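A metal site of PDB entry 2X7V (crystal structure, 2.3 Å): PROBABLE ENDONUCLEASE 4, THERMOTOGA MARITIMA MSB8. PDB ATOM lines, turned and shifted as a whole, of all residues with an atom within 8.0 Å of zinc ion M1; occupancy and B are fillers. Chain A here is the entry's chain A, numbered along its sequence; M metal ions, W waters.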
ATOM      1  N   HIS A  69     -38.590 -25.199 -35.907  1.00  0.00           N
ATOM      2  CA  HIS A  69     -37.880 -25.449 -34.672  1.00  0.00           C
ATOM      3  C   HIS A  69     -38.895 -25.463 -33.550  1.00  0.00           C
ATOM      4  O   HIS A  69     -39.733 -24.572 -33.494  1.00  0.00           O
ATOM      5  CB  HIS A  69     -36.833 -24.358 -34.431  1.00  0.00           C
ATOM      6  CG  HIS A  69     -35.886 -24.658 -33.320  1.00  0.00           C
ATOM      7  ND1 HIS A  69     -36.305 -24.981 -32.045  1.00  0.00           N
ATOM      8  CD2 HIS A  69     -34.530 -24.708 -33.293  1.00  0.00           C
ATOM      9  CE1 HIS A  69     -35.261 -25.216 -31.280  1.00  0.00           C
ATOM     10  NE2 HIS A  69     -34.174 -25.041 -32.005  1.00  0.00           N
ATOM     11  N   HIS A 109     -34.424 -29.980 -29.462  1.00  0.00           N
ATOM     12  CA  HIS A 109     -33.425 -30.383 -28.484  1.00  0.00           C
ATOM     13  C   HIS A 109     -33.977 -31.624 -27.822  1.00  0.00           C
ATOM     14  O   HIS A 109     -35.156 -31.666 -27.466  1.00  0.00           O
ATOM     15  CB  HIS A 109     -33.258 -29.282 -27.456  1.00  0.00           C
ATOM     16  CG  HIS A 109     -32.719 -28.004 -28.029  1.00  0.00           C
ATOM     17  ND1 HIS A 109     -32.143 -27.020 -27.258  1.00  0.00           N
ATOM     18  CD2 HIS A 109     -32.639 -27.574 -29.313  1.00  0.00           C
ATOM     19  CE1 HIS A 109     -31.744 -26.031 -28.038  1.00  0.00           C
ATOM     20  NE2 HIS A 109     -32.035 -26.342 -29.295  1.00  0.00           N
ATOM     21  N   GLU A 144     -30.984 -32.144 -32.374  1.00  0.00           N
ATOM     22  CA  GLU A 144     -29.922 -31.168 -32.386  1.00  0.00           C
ATOM     23  C   GLU A 144     -28.956 -31.376 -31.225  1.00  0.00           C
ATOM     24  O   GLU A 144     -29.388 -31.576 -30.094  1.00  0.00           O
ATOM     25  CB  GLU A 144     -30.513 -29.771 -32.297  1.00  0.00           C
ATOM     26  CG  GLU A 144     -29.442 -28.699 -32.371  1.00  0.00           C
ATOM     27  CD  GLU A 144     -29.991 -27.294 -32.183  1.00  0.00           C
ATOM     28  OE1 GLU A 144     -31.186 -27.050 -32.446  1.00  0.00           O
ATOM     29  OE2 GLU A 144     -29.220 -26.433 -31.770  1.00  0.00           O
ATOM     30  N   ASN A 145     -27.660 -31.332 -31.471  1.00  0.00           N
ATOM     31  CA  ASN A 145     -26.722 -31.363 -30.364  1.00  0.00           C
ATOM     32  C   ASN A 145     -26.879 -30.103 -29.497  1.00  0.00           C
ATOM     33  O   ASN A 145     -27.228 -29.035 -30.000  1.00  0.00           O
ATOM     34  CB  ASN A 145     -25.268 -31.556 -30.821  1.00  0.00           C
ATOM     35  CG  ASN A 145     -24.739 -30.396 -31.645  1.00  0.00           C
ATOM     36  OD1 ASN A 145     -23.749 -29.743 -31.280  1.00  0.00           O
ATOM     37  ND2 ASN A 145     -25.388 -30.130 -32.775  1.00  0.00           N
ATOM     38  N   VAL A 146     -26.666 -30.261 -28.189  1.00  0.00           N
ATOM     39  CA  VAL A 146     -26.812 -29.147 -27.259  1.00  0.00           C
ATOM     40  C   VAL A 146     -25.552 -28.963 -26.404  1.00  0.00           C
ATOM     41  O   VAL A 146     -24.605 -29.734 -26.488  1.00  0.00           O
ATOM     42  CB  VAL A 146     -28.046 -29.340 -26.339  1.00  0.00           C
ATOM     43  CG1 VAL A 146     -29.328 -29.273 -27.156  1.00  0.00           C
ATOM     44  CG2 VAL A 146     -27.945 -30.672 -25.577  1.00  0.00           C
ATOM     45  N   SER A 147     -25.558 -27.930 -25.563  1.00  0.00           N
ATOM     46  CA  SER A 147     -24.451 -27.735 -24.638  1.00  0.00           C
ATOM     47  C   SER A 147     -24.636 -28.600 -23.392  1.00  0.00           C
ATOM     48  O   SER A 147     -25.752 -29.023 -23.065  1.00  0.00           O
ATOM     49  CB  SER A 147     -24.341 -26.245 -24.263  1.00  0.00           C
ATOM     50  OG  SER A 147     -24.245 -25.437 -25.427  1.00  0.00           O
ATOM     51  N   ASP A 178     -25.197 -27.947 -34.461  1.00  0.00           N
ATOM     52  CA  ASP A 178     -25.109 -26.549 -34.086  1.00  0.00           C
ATOM     53  C   ASP A 178     -23.655 -26.303 -33.736  1.00  0.00           C
ATOM     54  O   ASP A 178     -23.108 -26.940 -32.823  1.00  0.00           O
ATOM     55  CB  ASP A 178     -26.036 -26.226 -32.908  1.00  0.00           C
ATOM     56  CG  ASP A 178     -25.985 -24.751 -32.482  1.00  0.00           C
ATOM     57  OD1 ASP A 178     -27.043 -24.111 -32.365  1.00  0.00           O
ATOM     58  OD2 ASP A 178     -24.889 -24.214 -32.258  1.00  0.00           O
ATOM     59  N   CYS A 180     -22.062 -23.775 -32.362  1.00  0.00           N
ATOM     60  CA  CYS A 180     -21.852 -23.227 -31.018  1.00  0.00           C
ATOM     61  C   CYS A 180     -21.987 -24.294 -29.911  1.00  0.00           C
ATOM     62  O   CYS A 180     -21.103 -24.427 -29.054  1.00  0.00           O
ATOM     63  CB  CYS A 180     -22.777 -22.029 -30.746  1.00  0.00           C
ATOM     64  SG  CYS A 180     -22.619 -21.406 -29.045  1.00  0.00           S
ATOM     65  N   HIS A 181     -23.062 -25.081 -29.939  1.00  0.00           N
ATOM     66  CA  HIS A 181     -23.208 -26.172 -28.970  1.00  0.00           C
ATOM     67  C   HIS A 181     -22.069 -27.198 -29.090  1.00  0.00           C
ATOM     68  O   HIS A 181     -21.565 -27.680 -28.083  1.00  0.00           O
ATOM     69  CB  HIS A 181     -24.560 -26.866 -29.130  1.00  0.00           C
ATOM     70  CG  HIS A 181     -25.729 -25.939 -29.011  1.00  0.00           C
ATOM     71  ND1 HIS A 181     -26.958 -26.216 -29.584  1.00  0.00           N
ATOM     72  CD2 HIS A 181     -25.865 -24.758 -28.387  1.00  0.00           C
ATOM     73  CE1 HIS A 181     -27.794 -25.239 -29.314  1.00  0.00           C
ATOM     74  NE2 HIS A 181     -27.158 -24.329 -28.595  1.00  0.00           N
ATOM     75  N   ASP A 184     -18.898 -25.685 -27.663  1.00  0.00           N
ATOM     76  CA  ASP A 184     -19.100 -25.769 -26.208  1.00  0.00           C
ATOM     77  C   ASP A 184     -18.737 -27.128 -25.648  1.00  0.00           C
ATOM     78  O   ASP A 184     -18.328 -27.234 -24.497  1.00  0.00           O
ATOM     79  CB  ASP A 184     -20.581 -25.569 -25.864  1.00  0.00           C
ATOM     80  CG  ASP A 184     -20.902 -24.190 -25.351  1.00  0.00           C
ATOM     81  OD1 ASP A 184     -19.981 -23.373 -25.082  1.00  0.00           O
ATOM     82  OD2 ASP A 184     -22.119 -23.905 -25.219  1.00  0.00           O
ATOM     83  N   HIS A 215     -26.733 -25.454 -37.655  1.00  0.00           N
ATOM     84  CA  HIS A 215     -26.933 -24.131 -37.086  1.00  0.00           C
ATOM     85  C   HIS A 215     -25.590 -23.436 -37.011  1.00  0.00           C
ATOM     86  O   HIS A 215     -24.696 -23.859 -36.294  1.00  0.00           O
ATOM     87  CB  HIS A 215     -27.601 -24.173 -35.722  1.00  0.00           C
ATOM     88  CG  HIS A 215     -29.033 -24.563 -35.766  1.00  0.00           C
ATOM     89  ND1 HIS A 215     -29.701 -25.077 -34.679  1.00  0.00           N
ATOM     90  CD2 HIS A 215     -29.925 -24.527 -36.782  1.00  0.00           C
ATOM     91  CE1 HIS A 215     -30.956 -25.328 -35.022  1.00  0.00           C
ATOM     92  NE2 HIS A 215     -31.112 -25.001 -36.287  1.00  0.00           N
ATOM     93  N   ASN A 217     -23.516 -20.852 -35.738  1.00  0.00           N
ATOM     94  CA  ASN A 217     -23.401 -19.903 -34.631  1.00  0.00           C
ATOM     95  C   ASN A 217     -21.934 -19.763 -34.198  1.00  0.00           C
ATOM     96  O   ASN A 217     -21.245 -20.760 -33.997  1.00  0.00           O
ATOM     97  CB  ASN A 217     -24.242 -20.362 -33.420  1.00  0.00           C
ATOM     98  CG  ASN A 217     -25.707 -20.539 -33.764  1.00  0.00           C
ATOM     99  OD1 ASN A 217     -26.316 -21.584 -33.474  1.00  0.00           O
ATOM    100  ND2 ASN A 217     -26.293 -19.520 -34.385  1.00  0.00           N
ATOM    101  N   LYS A 227     -21.309 -23.217 -22.223  1.00  0.00           N
ATOM    102  CA  LYS A 227     -21.997 -21.983 -21.827  1.00  0.00           C
ATOM    103  C   LYS A 227     -23.310 -21.689 -22.558  1.00  0.00           C
ATOM    104  O   LYS A 227     -24.190 -21.015 -22.023  1.00  0.00           O
ATOM    105  CB  LYS A 227     -21.053 -20.776 -21.977  1.00  0.00           C
ATOM    106  CG  LYS A 227     -19.919 -20.744 -20.970  1.00  0.00           C
ATOM    107  CD  LYS A 227     -20.422 -20.369 -19.585  1.00  0.00           C
ATOM    108  CE  LYS A 227     -19.269 -20.255 -18.599  1.00  0.00           C
ATOM    109  NZ  LYS A 227     -19.712 -20.015 -17.179  1.00  0.00           N
ATOM    110  N   ASP A 228     -23.435 -22.188 -23.787  1.00  0.00           N
ATOM    111  CA  ASP A 228     -24.623 -21.960 -24.599  1.00  0.00           C
ATOM    112  C   ASP A 228     -24.963 -20.474 -24.800  1.00  0.00           C
ATOM    113  O   ASP A 228     -26.089 -20.018 -24.527  1.00  0.00           O
ATOM    114  CB  ASP A 228     -25.816 -22.707 -24.015  1.00  0.00           C
ATOM    115  CG  ASP A 228     -26.986 -22.763 -24.968  1.00  0.00           C
ATOM    116  OD1 ASP A 228     -28.138 -22.912 -24.494  1.00  0.00           O
ATOM    117  OD2 ASP A 228     -26.740 -22.624 -26.191  1.00  0.00           O
ATOM    118  N   ARG A 229     -23.991 -19.707 -25.269  1.00  0.00           N
ATOM    119  CA  ARG A 229     -24.234 -18.326 -25.625  1.00  0.00           C
ATOM    120  C   ARG A 229     -23.743 -18.081 -27.058  1.00  0.00           C
ATOM    121  O   ARG A 229     -22.551 -18.087 -27.327  1.00  0.00           O
ATOM    122  CB  ARG A 229     -23.555 -17.377 -24.626  1.00  0.00           C
ATOM    123  CG  ARG A 229     -24.092 -17.429 -23.188  1.00  0.00           C
ATOM    124  CD  ARG A 229     -25.511 -16.834 -23.071  1.00  0.00           C
ATOM    125  NE  ARG A 229     -26.368 -17.671 -22.229  1.00  0.00           N
ATOM    126  CZ  ARG A 229     -26.903 -17.291 -21.077  1.00  0.00           C
ATOM    127  NH1 ARG A 229     -26.697 -16.066 -20.608  1.00  0.00           N
ATOM    128  NH2 ARG A 229     -27.657 -18.140 -20.374  1.00  0.00           N
ATOM    129  N   HIS A 230     -24.683 -17.886 -27.987  1.00  0.00           N
ATOM    130  CA  HIS A 230     -24.344 -17.674 -29.390  1.00  0.00           C
ATOM    131  C   HIS A 230     -23.737 -16.299 -29.636  1.00  0.00           C
ATOM    132  O   HIS A 230     -23.981 -15.359 -28.889  1.00  0.00           O
ATOM    133  CB  HIS A 230     -25.589 -17.772 -30.259  1.00  0.00           C
ATOM    134  CG  HIS A 230     -26.271 -19.100 -30.191  1.00  0.00           C
ATOM    135  ND1 HIS A 230     -27.403 -19.381 -30.938  1.00  0.00           N
ATOM    136  CD2 HIS A 230     -26.004 -20.213 -29.478  1.00  0.00           C
ATOM    137  CE1 HIS A 230     -27.796 -20.617 -30.678  1.00  0.00           C
ATOM    138  NE2 HIS A 230     -26.961 -21.147 -29.806  1.00  0.00           N
ATOM    139  N   GLU A 260     -28.416 -18.611 -36.166  1.00  0.00           N
ATOM    140  CA  GLU A 260     -29.228 -18.335 -34.981  1.00  0.00           C
ATOM    141  C   GLU A 260     -28.489 -17.356 -34.081  1.00  0.00           C
ATOM    142  O   GLU A 260     -28.584 -17.406 -32.868  1.00  0.00           O
ATOM    143  CB  GLU A 260     -29.492 -19.609 -34.189  1.00  0.00           C
ATOM    144  CG  GLU A 260     -30.227 -20.703 -34.929  1.00  0.00           C
ATOM    145  CD  GLU A 260     -30.434 -21.885 -34.023  1.00  0.00           C
ATOM    146  OE1 GLU A 260     -29.407 -22.374 -33.501  1.00  0.00           O
ATOM    147  OE2 GLU A 260     -31.600 -22.306 -33.794  1.00  0.00           O
HETATM  148 ZN    ZN M   1     -27.947 -22.357 -28.227  1.00  0.00          ZN
HETATM  149 ZN    ZN M   2     -29.129 -24.293 -32.514  1.00  0.00          ZN
HETATM  150 ZN    ZN M   3     -32.062 -25.371 -31.257  1.00  0.00          ZN
HETATM  151  O   HOH W   1     -30.108 -22.505 -29.266  1.00  0.00           O
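Zinc ion M1 is bound by a ring nitrogen (NE2) of His 181 (2.2 Å), a ring nitrogen (NE2) of His 230 (2.2 Å), the side-chain carboxylate (OD2) of Asp 228 (2.4 Å) and water W1 (2.4 Å).
The side-chain carboxylate of Asp 178 is in hydrogen-bond range of the backbone NH of His 181, at 3.1 Å. The side-chain carboxylate of Glu 144 sits close to a ring nitrogen (ND1) of His 181, at 3.2 Å. The backbone carbonyl oxygen (O) of Asn 145 sits at hydrogen-bond distance from a ring nitrogen (ND1) of His 181, 2.9 Å away. The backbone carbonyl oxygen of Glu 260 sits at hydrogen-bond distance from a ring nitrogen (ND1) of His 230 (3.0 Å). The backbone NH of Asp 228 sits at hydrogen-bond distance from the side-chain carboxylate of Asp 184, 2.6 Å away.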
